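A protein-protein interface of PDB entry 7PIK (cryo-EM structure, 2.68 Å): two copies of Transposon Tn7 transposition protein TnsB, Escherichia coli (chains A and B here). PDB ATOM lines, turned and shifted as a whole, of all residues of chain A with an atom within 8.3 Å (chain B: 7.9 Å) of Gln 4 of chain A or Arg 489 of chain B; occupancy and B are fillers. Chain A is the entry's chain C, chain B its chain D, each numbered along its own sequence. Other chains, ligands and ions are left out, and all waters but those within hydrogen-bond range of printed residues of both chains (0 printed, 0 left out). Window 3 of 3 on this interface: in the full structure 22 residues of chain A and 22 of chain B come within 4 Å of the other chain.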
ATOM      1  N   MET A   2     -23.919  -5.529 -24.030  1.00  0.00           N
ATOM      2  CA  MET A   2     -22.697  -5.123 -24.713  1.00  0.00           C
ATOM      3  C   MET A   2     -22.254  -6.179 -25.719  1.00  0.00           C
ATOM      4  O   MET A   2     -22.665  -6.156 -26.878  1.00  0.00           O
ATOM      5  CB  MET A   2     -21.581  -4.856 -23.702  1.00  0.00           C
ATOM      6  N   TRP A   3     -21.412  -7.105 -25.266  1.00  0.00           N
ATOM      7  CA  TRP A   3     -20.911  -8.185 -26.102  1.00  0.00           C
ATOM      8  C   TRP A   3     -21.059  -9.511 -25.372  1.00  0.00           C
ATOM      9  O   TRP A   3     -21.151  -9.565 -24.143  1.00  0.00           O
ATOM     10  CB  TRP A   3     -19.440  -7.978 -26.487  1.00  0.00           C
ATOM     11  CG  TRP A   3     -19.209  -6.854 -27.443  1.00  0.00           C
ATOM     12  CD1 TRP A   3     -19.588  -6.799 -28.751  1.00  0.00           C
ATOM     13  CD2 TRP A   3     -18.537  -5.621 -27.166  1.00  0.00           C
ATOM     14  NE1 TRP A   3     -19.197  -5.606 -29.307  1.00  0.00           N
ATOM     15  CE2 TRP A   3     -18.549  -4.865 -28.354  1.00  0.00           C
ATOM     16  CE3 TRP A   3     -17.929  -5.083 -26.029  1.00  0.00           C
ATOM     17  CZ2 TRP A   3     -17.978  -3.600 -28.437  1.00  0.00           C
ATOM     18  CZ3 TRP A   3     -17.362  -3.826 -26.114  1.00  0.00           C
ATOM     19  CH2 TRP A   3     -17.391  -3.099 -27.308  1.00  0.00           C
ATOM     20  N   GLN A   4     -21.083 -10.584 -26.151  1.00  0.00           N
ATOM     21  CA  GLN A   4     -21.089 -11.940 -25.626  1.00  0.00           C
ATOM     22  C   GLN A   4     -19.683 -12.527 -25.673  1.00  0.00           C
ATOM     23  O   GLN A   4     -18.751 -11.940 -26.226  1.00  0.00           O
ATOM     24  CB  GLN A   4     -22.061 -12.820 -26.416  1.00  0.00           C
ATOM     25  CG  GLN A   4     -23.475 -12.820 -25.879  1.00  0.00           C
ATOM     26  CD  GLN A   4     -24.468 -13.375 -26.875  1.00  0.00           C
ATOM     27  OE1 GLN A   4     -24.274 -13.271 -28.085  1.00  0.00           O
ATOM     28  NE2 GLN A   4     -25.543 -13.969 -26.370  1.00  0.00           N
ATOM     29  N   ILE A   5     -19.538 -13.698 -25.076  1.00  0.00           N
ATOM     30  CA  ILE A   5     -18.283 -14.435 -25.143  1.00  0.00           C
ATOM     31  C   ILE A   5     -18.226 -15.188 -26.464  1.00  0.00           C
ATOM     32  O   ILE A   5     -19.237 -15.728 -26.930  1.00  0.00           O
ATOM     33  CB  ILE A   5     -18.152 -15.386 -23.939  1.00  0.00           C
ATOM     34  CG1 ILE A   5     -18.180 -14.598 -22.630  1.00  0.00           C
ATOM     35  CG2 ILE A   5     -16.875 -16.201 -24.024  1.00  0.00           C
ATOM     36  CD1 ILE A   5     -17.264 -13.403 -22.617  1.00  0.00           C
ATOM     37  N   ASN A   6     -17.042 -15.202 -27.083  1.00  0.00           N
ATOM     38  CA  ASN A   6     -16.774 -15.953 -28.313  1.00  0.00           C
ATOM     39  C   ASN A   6     -17.498 -15.359 -29.519  1.00  0.00           C
ATOM     40  O   ASN A   6     -18.049 -16.086 -30.344  1.00  0.00           O
ATOM     41  CB  ASN A   6     -17.128 -17.436 -28.158  1.00  0.00           C
ATOM     42  CG  ASN A   6     -16.141 -18.183 -27.298  1.00  0.00           C
ATOM     43  OD1 ASN A   6     -14.952 -17.881 -27.294  1.00  0.00           O
ATOM     44  ND2 ASN A   6     -16.630 -19.167 -26.557  1.00  0.00           N
ATOM     45  N   GLU A   7     -17.486 -14.036 -29.637  1.00  0.00           N
ATOM     46  CA  GLU A   7     -18.090 -13.357 -30.772  1.00  0.00           C
ATOM     47  C   GLU A   7     -17.036 -12.531 -31.499  1.00  0.00           C
ATOM     48  O   GLU A   7     -16.120 -11.979 -30.883  1.00  0.00           O
ATOM     49  CB  GLU A   7     -19.283 -12.492 -30.322  1.00  0.00           C
ATOM     50  CG  GLU A   7     -18.953 -11.381 -29.344  1.00  0.00           C
ATOM     51  CD  GLU A   7     -18.504 -10.111 -30.027  1.00  0.00           C
ATOM     52  OE1 GLU A   7     -18.794  -9.950 -31.231  1.00  0.00           O
ATOM     53  OE2 GLU A   7     -17.863  -9.273 -29.365  1.00  0.00           O
ATOM     54  N   VAL A   8     -17.167 -12.464 -32.822  1.00  0.00           N
ATOM     55  CA  VAL A   8     -16.137 -11.927 -33.705  1.00  0.00           C
ATOM     56  C   VAL A   8     -16.563 -10.554 -34.203  1.00  0.00           C
ATOM     57  O   VAL A   8     -17.746 -10.318 -34.475  1.00  0.00           O
ATOM     58  CB  VAL A   8     -15.872 -12.885 -34.884  1.00  0.00           C
ATOM     59  CG1 VAL A   8     -14.684 -12.416 -35.709  1.00  0.00           C
ATOM     60  CG2 VAL A   8     -15.644 -14.299 -34.374  1.00  0.00           C
ATOM     61  N   VAL A   9     -15.594  -9.642 -34.305  1.00  0.00           N
ATOM     62  CA  VAL A   9     -15.820  -8.290 -34.803  1.00  0.00           C
ATOM     63  C   VAL A   9     -14.722  -7.925 -35.794  1.00  0.00           C
ATOM     64  O   VAL A   9     -13.632  -8.498 -35.791  1.00  0.00           O
ATOM     65  CB  VAL A   9     -15.873  -7.247 -33.663  1.00  0.00           C
ATOM     66  CG1 VAL A   9     -16.941  -7.614 -32.644  1.00  0.00           C
ATOM     67  CG2 VAL A   9     -14.518  -7.124 -32.991  1.00  0.00           C
ATOM     68  N   ARG A  17     -11.641 -11.930 -31.945  1.00  0.00           N
ATOM     69  CA  ARG A  17     -12.571 -12.693 -31.123  1.00  0.00           C
ATOM     70  C   ARG A  17     -12.410 -12.298 -29.664  1.00  0.00           C
ATOM     71  O   ARG A  17     -11.283 -12.229 -29.157  1.00  0.00           O
ATOM     72  CB  ARG A  17     -12.353 -14.201 -31.275  1.00  0.00           C
ATOM     73  CG  ARG A  17     -13.460 -15.051 -30.659  1.00  0.00           C
ATOM     74  CD  ARG A  17     -13.117 -16.530 -30.659  1.00  0.00           C
ATOM     75  NE  ARG A  17     -13.070 -17.087 -32.005  1.00  0.00           N
ATOM     76  CZ  ARG A  17     -14.111 -17.611 -32.635  1.00  0.00           C
ATOM     77  NH1 ARG A  17     -15.301 -17.678 -32.066  1.00  0.00           N
ATOM     78  NH2 ARG A  17     -13.952 -18.080 -33.869  1.00  0.00           N
ATOM     79  N   ILE A  18     -13.538 -12.064 -28.995  1.00  0.00           N
ATOM     80  CA  ILE A  18     -13.557 -11.718 -27.577  1.00  0.00           C
ATOM     81  C   ILE A  18     -13.458 -12.995 -26.754  1.00  0.00           C
ATOM     82  O   ILE A  18     -14.241 -13.933 -26.944  1.00  0.00           O
ATOM     83  CB  ILE A  18     -14.834 -10.937 -27.224  1.00  0.00           C
ATOM     84  CG1 ILE A  18     -14.998  -9.718 -28.136  1.00  0.00           C
ATOM     85  CG2 ILE A  18     -14.831 -10.534 -25.757  1.00  0.00           C
ATOM     86  CD1 ILE A  18     -13.951  -8.653 -27.940  1.00  0.00           C
ATOM     87  N   LEU A  19     -12.501 -13.035 -25.829  1.00  0.00           N
ATOM     88  CA  LEU A  19     -12.279 -14.216 -25.011  1.00  0.00           C
ATOM     89  C   LEU A  19     -12.885 -14.101 -23.622  1.00  0.00           C
ATOM     90  O   LEU A  19     -13.485 -15.063 -23.135  1.00  0.00           O
ATOM     91  CB  LEU A  19     -10.778 -14.495 -24.889  1.00  0.00           C
ATOM     92  CG  LEU A  19     -10.007 -14.713 -26.193  1.00  0.00           C
ATOM     93  CD1 LEU A  19      -8.548 -14.992 -25.901  1.00  0.00           C
ATOM     94  CD2 LEU A  19     -10.617 -15.838 -27.007  1.00  0.00           C
ATOM     95  N   ALA A  20     -12.746 -12.951 -22.970  1.00  0.00           N
ATOM     96  CA  ALA A  20     -13.282 -12.765 -21.631  1.00  0.00           C
ATOM     97  C   ALA A  20     -13.687 -11.311 -21.450  1.00  0.00           C
ATOM     98  O   ALA A  20     -13.045 -10.408 -21.991  1.00  0.00           O
ATOM     99  CB  ALA A  20     -12.266 -13.168 -20.557  1.00  0.00           C
ATOM    100  N   ILE A  21     -14.759 -11.097 -20.693  1.00  0.00           N
ATOM    101  CA  ILE A  21     -15.227  -9.766 -20.327  1.00  0.00           C
ATOM    102  C   ILE A  21     -15.258  -9.687 -18.810  1.00  0.00           C
ATOM    103  O   ILE A  21     -15.852 -10.547 -18.150  1.00  0.00           O
ATOM    104  CB  ILE A  21     -16.612  -9.457 -20.925  1.00  0.00           C
ATOM    105  CG1 ILE A  21     -16.480  -9.037 -22.390  1.00  0.00           C
ATOM    106  CG2 ILE A  21     -17.308  -8.368 -20.130  1.00  0.00           C
ATOM    107  CD1 ILE A  21     -17.745  -9.219 -23.190  1.00  0.00           C
ATOM    108  N   VAL A  26     -11.433  -5.816 -21.126  1.00  0.00           N
ATOM    109  CA  VAL A  26     -11.878  -6.733 -22.169  1.00  0.00           C
ATOM    110  C   VAL A  26     -10.649  -7.346 -22.827  1.00  0.00           C
ATOM    111  O   VAL A  26      -9.713  -6.627 -23.198  1.00  0.00           O
ATOM    112  CB  VAL A  26     -12.766  -6.034 -23.216  1.00  0.00           C
ATOM    113  CG1 VAL A  26     -12.835  -6.853 -24.491  1.00  0.00           C
ATOM    114  CG2 VAL A  26     -14.159  -5.827 -22.663  1.00  0.00           C
ATOM    115  N   VAL A  27     -10.595  -8.697 -22.857  1.00  0.00           N
ATOM    116  CA  VAL A  27      -9.491  -9.473 -23.498  1.00  0.00           C
ATOM    117  C   VAL A  27      -9.883 -10.044 -24.858  1.00  0.00           C
ATOM    118  O   VAL A  27     -10.890 -10.697 -24.969  1.00  0.00           O
ATOM    119  CB  VAL A  27      -9.039 -10.655 -22.630  1.00  0.00           C
ATOM    120  CG1 VAL A  27      -7.706 -11.208 -23.100  1.00  0.00           C
ATOM    121  CG2 VAL A  27      -8.984 -10.259 -21.167  1.00  0.00           C
ATOM    122  N   ARG A  57     -19.796  -5.491 -36.407  1.00  0.00           N
ATOM    123  CA  ARG A  57     -20.152  -6.853 -36.041  1.00  0.00           C
ATOM    124  C   ARG A  57     -20.071  -7.774 -37.252  1.00  0.00           C
ATOM    125  O   ARG A  57     -20.189  -7.335 -38.399  1.00  0.00           O
ATOM    126  CB  ARG A  57     -21.559  -6.893 -35.445  1.00  0.00           C
ATOM    127  CG  ARG A  57     -21.783  -5.880 -34.336  1.00  0.00           C
ATOM    128  CD  ARG A  57     -22.888  -6.326 -33.395  1.00  0.00           C
ATOM    129  NE  ARG A  57     -22.769  -5.703 -32.083  1.00  0.00           N
ATOM    130  CZ  ARG A  57     -23.599  -5.923 -31.072  1.00  0.00           C
ATOM    131  NH1 ARG A  57     -24.628  -6.745 -31.190  1.00  0.00           N
ATOM    132  NH2 ARG A  57     -23.389  -5.303 -29.914  1.00  0.00           N
ATOM    133  N   GLY A 131     -12.550 -21.040 -30.985  1.00  0.00           N
ATOM    134  CA  GLY A 131     -13.852 -20.921 -30.359  1.00  0.00           C
ATOM    135  C   GLY A 131     -13.995 -21.500 -28.969  1.00  0.00           C
ATOM    136  O   GLY A 131     -15.117 -21.641 -28.475  1.00  0.00           O
ATOM    137  N   GLN A 132     -12.878 -21.856 -28.336  1.00  0.00           N
ATOM    138  CA  GLN A 132     -12.850 -22.256 -26.928  1.00  0.00           C
ATOM    139  C   GLN A 132     -13.711 -23.493 -26.665  1.00  0.00           C
ATOM    140  O   GLN A 132     -14.500 -23.541 -25.720  1.00  0.00           O
ATOM    141  CB  GLN A 132     -13.267 -21.093 -26.026  1.00  0.00           C
ATOM    142  CG  GLN A 132     -12.193 -20.036 -25.852  1.00  0.00           C
ATOM    143  CD  GLN A 132     -12.630 -18.891 -24.962  1.00  0.00           C
ATOM    144  OE1 GLN A 132     -12.050 -18.654 -23.906  1.00  0.00           O
ATOM    145  NE2 GLN A 132     -13.655 -18.169 -25.390  1.00  0.00           N
ATOM    146  N   THR A 133     -13.545 -24.505 -27.507  1.00  0.00           N
ATOM    147  CA  THR A 133     -14.202 -25.794 -27.361  1.00  0.00           C
ATOM    148  C   THR A 133     -13.192 -26.907 -27.600  1.00  0.00           C
ATOM    149  O   THR A 133     -12.187 -26.691 -28.280  1.00  0.00           O
ATOM    150  CB  THR A 133     -15.371 -25.943 -28.350  1.00  0.00           C
ATOM    151  OG1 THR A 133     -14.973 -25.472 -29.645  1.00  0.00           O
ATOM    152  CG2 THR A 133     -16.586 -25.159 -27.874  1.00  0.00           C
ATOM    153  N   GLY B 268     -26.075 -17.721 -14.714  1.00  0.00           N
ATOM    154  CA  GLY B 268     -25.590 -18.517 -15.817  1.00  0.00           C
ATOM    155  C   GLY B 268     -24.474 -19.481 -15.489  1.00  0.00           C
ATOM    156  O   GLY B 268     -23.813 -19.970 -16.410  1.00  0.00           O
ATOM    157  N   CYS B 331     -32.509 -21.157 -23.874  1.00  0.00           N
ATOM    158  CA  CYS B 331     -31.367 -20.473 -24.457  1.00  0.00           C
ATOM    159  C   CYS B 331     -31.743 -19.546 -25.606  1.00  0.00           C
ATOM    160  O   CYS B 331     -30.852 -18.955 -26.220  1.00  0.00           O
ATOM    161  CB  CYS B 331     -30.332 -21.502 -24.931  1.00  0.00           C
ATOM    162  SG  CYS B 331     -29.566 -22.461 -23.599  1.00  0.00           S
ATOM    163  N   CYS B 352     -32.857 -13.372 -20.745  1.00  0.00           N
ATOM    164  CA  CYS B 352     -32.240 -14.700 -20.652  1.00  0.00           C
ATOM    165  C   CYS B 352     -31.882 -15.340 -22.001  1.00  0.00           C
ATOM    166  O   CYS B 352     -32.537 -16.297 -22.416  1.00  0.00           O
ATOM    167  CB  CYS B 352     -33.167 -15.643 -19.881  1.00  0.00           C
ATOM    168  SG  CYS B 352     -32.979 -15.627 -18.084  1.00  0.00           S
ATOM    169  N   VAL B 353     -30.849 -14.834 -22.680  1.00  0.00           N
ATOM    170  CA  VAL B 353     -30.436 -15.392 -23.962  1.00  0.00           C
ATOM    171  C   VAL B 353     -28.973 -15.788 -23.840  1.00  0.00           C
ATOM    172  O   VAL B 353     -28.152 -14.999 -23.360  1.00  0.00           O
ATOM    173  CB  VAL B 353     -30.631 -14.396 -25.126  1.00  0.00           C
ATOM    174  CG1 VAL B 353     -30.069 -14.964 -26.418  1.00  0.00           C
ATOM    175  CG2 VAL B 353     -32.098 -14.044 -25.300  1.00  0.00           C
ATOM    176  N   GLY B 354     -28.641 -17.003 -24.267  1.00  0.00           N
ATOM    177  CA  GLY B 354     -27.280 -17.486 -24.231  1.00  0.00           C
ATOM    178  C   GLY B 354     -27.195 -18.849 -23.589  1.00  0.00           C
ATOM    179  O   GLY B 354     -28.205 -19.470 -23.247  1.00  0.00           O
ATOM    180  N   LEU B 355     -25.959 -19.318 -23.412  1.00  0.00           N
ATOM    181  CA  LEU B 355     -25.618 -20.650 -22.948  1.00  0.00           C
ATOM    182  C   LEU B 355     -25.003 -20.608 -21.556  1.00  0.00           C
ATOM    183  O   LEU B 355     -24.120 -19.786 -21.295  1.00  0.00           O
ATOM    184  CB  LEU B 355     -24.627 -21.320 -23.906  1.00  0.00           C
ATOM    185  CG  LEU B 355     -25.168 -22.096 -25.101  1.00  0.00           C
ATOM    186  CD1 LEU B 355     -24.008 -22.585 -25.946  1.00  0.00           C
ATOM    187  CD2 LEU B 355     -26.029 -23.258 -24.646  1.00  0.00           C
ATOM    188  N   PRO B 356     -25.436 -21.486 -20.649  1.00  0.00           N
ATOM    189  CA  PRO B 356     -24.843 -21.521 -19.307  1.00  0.00           C
ATOM    190  C   PRO B 356     -23.526 -22.281 -19.257  1.00  0.00           C
ATOM    191  O   PRO B 356     -23.002 -22.707 -20.291  1.00  0.00           O
ATOM    192  CB  PRO B 356     -25.923 -22.224 -18.483  1.00  0.00           C
ATOM    193  CG  PRO B 356     -26.524 -23.166 -19.450  1.00  0.00           C
ATOM    194  CD  PRO B 356     -26.541 -22.450 -20.777  1.00  0.00           C
ATOM    195  N   ASP B 357     -22.983 -22.452 -18.053  1.00  0.00           N
ATOM    196  CA  ASP B 357     -21.724 -23.160 -17.853  1.00  0.00           C
ATOM    197  C   ASP B 357     -21.929 -24.639 -17.534  1.00  0.00           C
ATOM    198  O   ASP B 357     -21.272 -25.498 -18.127  1.00  0.00           O
ATOM    199  CB  ASP B 357     -20.922 -22.495 -16.731  1.00  0.00           C
ATOM    200  CG  ASP B 357     -20.214 -21.239 -17.183  1.00  0.00           C
ATOM    201  OD1 ASP B 357     -20.226 -20.947 -18.396  1.00  0.00           O
ATOM    202  OD2 ASP B 357     -19.645 -20.539 -16.322  1.00  0.00           O
ATOM    203  N   VAL B 358     -22.822 -24.949 -16.596  1.00  0.00           N
ATOM    204  CA  VAL B 358     -23.037 -26.312 -16.122  1.00  0.00           C
ATOM    205  C   VAL B 358     -24.533 -26.593 -16.092  1.00  0.00           C
ATOM    206  O   VAL B 358     -25.332 -25.707 -15.770  1.00  0.00           O
ATOM    207  CB  VAL B 358     -22.413 -26.532 -14.725  1.00  0.00           C
ATOM    208  CG1 VAL B 358     -22.631 -27.957 -14.251  1.00  0.00           C
ATOM    209  CG2 VAL B 358     -20.934 -26.208 -14.744  1.00  0.00           C
ATOM    210  N   LEU B 374     -23.583 -32.096 -26.230  1.00  0.00           N
ATOM    211  CA  LEU B 374     -23.515 -31.096 -25.171  1.00  0.00           C
ATOM    212  C   LEU B 374     -22.080 -30.852 -24.720  1.00  0.00           C
ATOM    213  O   LEU B 374     -21.685 -29.706 -24.481  1.00  0.00           O
ATOM    214  CB  LEU B 374     -24.379 -31.525 -23.986  1.00  0.00           C
ATOM    215  CG  LEU B 374     -25.817 -31.008 -23.978  1.00  0.00           C
ATOM    216  CD1 LEU B 374     -26.578 -31.578 -22.797  1.00  0.00           C
ATOM    217  CD2 LEU B 374     -25.843 -29.489 -23.956  1.00  0.00           C
ATOM    218  N   PHE B 378     -20.700 -27.940 -27.857  1.00  0.00           N
ATOM    219  CA  PHE B 378     -21.170 -26.699 -27.265  1.00  0.00           C
ATOM    220  C   PHE B 378     -20.516 -26.377 -25.932  1.00  0.00           C
ATOM    221  O   PHE B 378     -20.738 -25.279 -25.407  1.00  0.00           O
ATOM    222  CB  PHE B 378     -22.698 -26.734 -27.092  1.00  0.00           C
ATOM    223  CG  PHE B 378     -23.446 -26.951 -28.378  1.00  0.00           C
ATOM    224  CD1 PHE B 378     -23.616 -25.916 -29.279  1.00  0.00           C
ATOM    225  CD2 PHE B 378     -23.967 -28.193 -28.692  1.00  0.00           C
ATOM    226  CE1 PHE B 378     -24.291 -26.116 -30.463  1.00  0.00           C
ATOM    227  CE2 PHE B 378     -24.645 -28.397 -29.876  1.00  0.00           C
ATOM    228  CZ  PHE B 378     -24.807 -27.359 -30.761  1.00  0.00           C
ATOM    229  N   ASN B 379     -19.723 -27.292 -25.374  1.00  0.00           N
ATOM    230  CA  ASN B 379     -18.943 -27.066 -24.157  1.00  0.00           C
ATOM    231  C   ASN B 379     -19.839 -26.703 -22.969  1.00  0.00           C
ATOM    232  O   ASN B 379     -19.705 -25.648 -22.347  1.00  0.00           O
ATOM    233  CB  ASN B 379     -17.867 -25.999 -24.387  1.00  0.00           C
ATOM    234  CG  ASN B 379     -16.659 -26.182 -23.486  1.00  0.00           C
ATOM    235  OD1 ASN B 379     -16.556 -27.167 -22.758  1.00  0.00           O
ATOM    236  ND2 ASN B 379     -15.740 -25.228 -23.530  1.00  0.00           N
ATOM    237  N   VAL B 380     -20.760 -27.611 -22.660  1.00  0.00           N
ATOM    238  CA  VAL B 380     -21.588 -27.534 -21.463  1.00  0.00           C
ATOM    239  C   VAL B 380     -21.293 -28.762 -20.615  1.00  0.00           C
ATOM    240  O   VAL B 380     -21.410 -29.895 -21.094  1.00  0.00           O
ATOM    241  CB  VAL B 380     -23.088 -27.450 -21.802  1.00  0.00           C
ATOM    242  CG1 VAL B 380     -23.906 -27.230 -20.544  1.00  0.00           C
ATOM    243  CG2 VAL B 380     -23.354 -26.340 -22.806  1.00  0.00           C
ATOM    244  N   ARG B 381     -20.908 -28.541 -19.363  1.00  0.00           N
ATOM    245  CA  ARG B 381     -20.575 -29.631 -18.460  1.00  0.00           C
ATOM    246  C   ARG B 381     -21.830 -30.172 -17.788  1.00  0.00           C
ATOM    247  O   ARG B 381     -22.673 -29.408 -17.313  1.00  0.00           O
ATOM    248  CB  ARG B 381     -19.572 -29.167 -17.404  1.00  0.00           C
ATOM    249  CG  ARG B 381     -18.241 -28.717 -17.974  1.00  0.00           C
ATOM    250  CD  ARG B 381     -17.240 -28.420 -16.873  1.00  0.00           C
ATOM    251  NE  ARG B 381     -17.274 -27.020 -16.466  1.00  0.00           N
ATOM    252  CZ  ARG B 381     -17.442 -26.607 -15.217  1.00  0.00           C
ATOM    253  NH1 ARG B 381     -17.585 -27.465 -14.220  1.00  0.00           N
ATOM    254  NH2 ARG B 381     -17.466 -25.303 -14.964  1.00  0.00           N
ATOM    255  N   GLY B 486     -20.459 -11.244 -16.170  1.00  0.00           N
ATOM    256  CA  GLY B 486     -20.255 -10.643 -17.471  1.00  0.00           C
ATOM    257  C   GLY B 486     -21.447 -10.863 -18.378  1.00  0.00           C
ATOM    258  O   GLY B 486     -22.451 -10.154 -18.271  1.00  0.00           O
ATOM    259  N   SER B 487     -21.342 -11.833 -19.286  1.00  0.00           N
ATOM    260  CA  SER B 487     -22.443 -12.194 -20.168  1.00  0.00           C
ATOM    261  C   SER B 487     -22.475 -13.709 -20.327  1.00  0.00           C
ATOM    262  O   SER B 487     -21.704 -14.439 -19.698  1.00  0.00           O
ATOM    263  CB  SER B 487     -22.316 -11.489 -21.524  1.00  0.00           C
ATOM    264  OG  SER B 487     -21.113 -11.851 -22.175  1.00  0.00           O
ATOM    265  N   LEU B 488     -23.389 -14.182 -21.171  1.00  0.00           N
ATOM    266  CA  LEU B 488     -23.488 -15.592 -21.514  1.00  0.00           C
ATOM    267  C   LEU B 488     -22.718 -15.845 -22.810  1.00  0.00           C
ATOM    268  O   LEU B 488     -21.983 -14.983 -23.298  1.00  0.00           O
ATOM    269  CB  LEU B 488     -24.953 -16.011 -21.617  1.00  0.00           C
ATOM    270  CG  LEU B 488     -25.780 -16.025 -20.327  1.00  0.00           C
ATOM    271  CD1 LEU B 488     -27.220 -16.374 -20.630  1.00  0.00           C
ATOM    272  CD2 LEU B 488     -25.208 -16.995 -19.311  1.00  0.00           C
ATOM    273  N   ARG B 489     -22.877 -17.032 -23.384  1.00  0.00           N
ATOM    274  CA  ARG B 489     -22.142 -17.427 -24.576  1.00  0.00           C
ATOM    275  C   ARG B 489     -23.072 -17.511 -25.779  1.00  0.00           C
ATOM    276  O   ARG B 489     -24.286 -17.673 -25.648  1.00  0.00           O
ATOM    277  CB  ARG B 489     -21.437 -18.769 -24.359  1.00  0.00           C
ATOM    278  CG  ARG B 489     -20.417 -18.743 -23.239  1.00  0.00           C
ATOM    279  CD  ARG B 489     -19.442 -19.889 -23.357  1.00  0.00           C
ATOM    280  NE  ARG B 489     -20.116 -21.179 -23.313  1.00  0.00           N
ATOM    281  CZ  ARG B 489     -20.118 -21.989 -22.263  1.00  0.00           C
ATOM    282  NH1 ARG B 489     -19.475 -21.676 -21.150  1.00  0.00           N
ATOM    283  NH2 ARG B 489     -20.779 -23.139 -22.332  1.00  0.00           N
ATOM    284  N   ALA B 490     -22.478 -17.397 -26.963  1.00  0.00           N
ATOM    285  CA  ALA B 490     -23.237 -17.371 -28.202  1.00  0.00           C
ATOM    286  C   ALA B 490     -23.669 -18.773 -28.615  1.00  0.00           C
ATOM    287  O   ALA B 490     -22.996 -19.765 -28.326  1.00  0.00           O
ATOM    288  CB  ALA B 490     -22.411 -16.732 -29.318  1.00  0.00           C
ATOM    289  N   VAL B 491     -24.809 -18.843 -29.302  1.00  0.00           N
ATOM    290  CA  VAL B 491     -25.366 -20.107 -29.774  1.00  0.00           C
ATOM    291  C   VAL B 491     -26.429 -19.783 -30.812  1.00  0.00           C
ATOM    292  O   VAL B 491     -27.026 -18.704 -30.794  1.00  0.00           O
ATOM    293  CB  VAL B 491     -25.939 -20.941 -28.598  1.00  0.00           C
ATOM    294  CG1 VAL B 491     -27.151 -20.256 -27.981  1.00  0.00           C
ATOM    295  CG2 VAL B 491     -26.274 -22.359 -29.042  1.00  0.00           C
ATOM    296  N   GLU B 492     -26.660 -20.719 -31.731  1.00  0.00           N
ATOM    297  CA  GLU B 492     -27.736 -20.608 -32.706  1.00  0.00           C
ATOM    298  C   GLU B 492     -28.695 -21.778 -32.538  1.00  0.00           C
ATOM    299  O   GLU B 492     -28.277 -22.905 -32.259  1.00  0.00           O
ATOM    300  CB  GLU B 492     -27.191 -20.543 -34.138  1.00  0.00           C
ATOM    301  CG  GLU B 492     -26.486 -21.785 -34.625  1.00  0.00           C
ATOM    302  CD  GLU B 492     -25.882 -21.590 -36.001  1.00  0.00           C
ATOM    303  OE1 GLU B 492     -25.000 -20.717 -36.142  1.00  0.00           O
ATOM    304  OE2 GLU B 492     -26.295 -22.296 -36.944  1.00  0.00           O
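Printed residues of chain B that touch a printed residue of chain A: Asn 379, Ser 487, Leu 488, Arg 489 and Ala 490.
Of the 19 printed residues of chain A, 5 touch a printed residue of chain B.
Hydrophobic or aromatic side chains of chain A that line the printed part of chain B: Ile 5.
Among the printed residues, 9 pairs touch across the chains.
Among the printed residues, no Asp or Glu carboxylate lies within 4 Å of a Lys or Arg side-chain nitrogen of the other chain.
ND2 of Asn 6 of chain A sits close to NE2 of Gln 132 of chain A.
O of Arg 489 of chain B lies within hydrogen-bond range of N of Leu 355 of chain B, at 3.2 Å.
The backbone carbonyl oxygen of Pro 356 of chain B is in hydrogen-bond range of the guanidinium group of Arg 489 of chain B.
The side-chain carboxylate (OD1) of Asp 357 of chain B lies within salt-bridge range of the guanidinium group (NH1) of Arg 489 of chain B (2.9 Å).
The backbone carbonyl oxygen (O) of Leu 374 of chain B is in hydrogen-bond range of the backbone NH (N) of Asn 379 of chain B (3.2 Å).
The backbone carbonyl oxygen (O) of Asn 379 of chain B is in hydrogen-bond range of the guanidinium group (NH2) of Arg 489 of chain B, at 2.7 Å.
Among the printed residues, pairs that only touch across the chains: Gln 4 of chain A with Ser 487 of chain B, Gln 4 of chain A with Leu 488 of chain B, Gln 4 of chain A with Arg 489 of chain B, Ile 5 of chain A with Ser 487 of chain B, Ile 5 of chain A with Ala 490 of chain B and Thr 133 of chain A with Asn 379 of chain B.
No position is printed for both chains.
The side-chain hydroxyl (OG) of Ser 487 of chain B sits at hydrogen-bond distance from the backbone carbonyl oxygen (O) of Trp 3 of chain A.
The backbone carbonyl oxygen of Leu 488 of chain B is in hydrogen-bond range of the backbone NH of Ile 5 of chain A (3.3 Å).
The side-chain amide nitrogen of Asn 379 of chain B sits at hydrogen-bond distance from the backbone carbonyl oxygen of Gln 132 of chain A (3.0 Å).
Of chain B, only Ser 487, Leu 488 and Arg 489 come within 4 Å of Gln 4 of chain A.
Arg 489 of chain B touches one residue of chain A.
Of chain A, only Ile 5 (3.6 Å) comes within 4 Å of Ala 490 of chain B.
Of the printed residues of chain A, Leu 488 of chain B touches Gln 4 (3.7 Å) and Ile 5 (3.3 Å).
Of the printed residues of chain B, Trp 3 of chain A touches Ser 487.
Printed residues of chain B within 4 Å of Thr 133 of chain A: Asn 379.
Leu 374 of chain B touches none of the printed residues of chain A.
Arg 57 of chain A touches none of the printed residues of chain B.
The nearest printed residue of chain A that does not touch Ser 487 of chain B is Ile 21 of chain A (4.4 Å).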
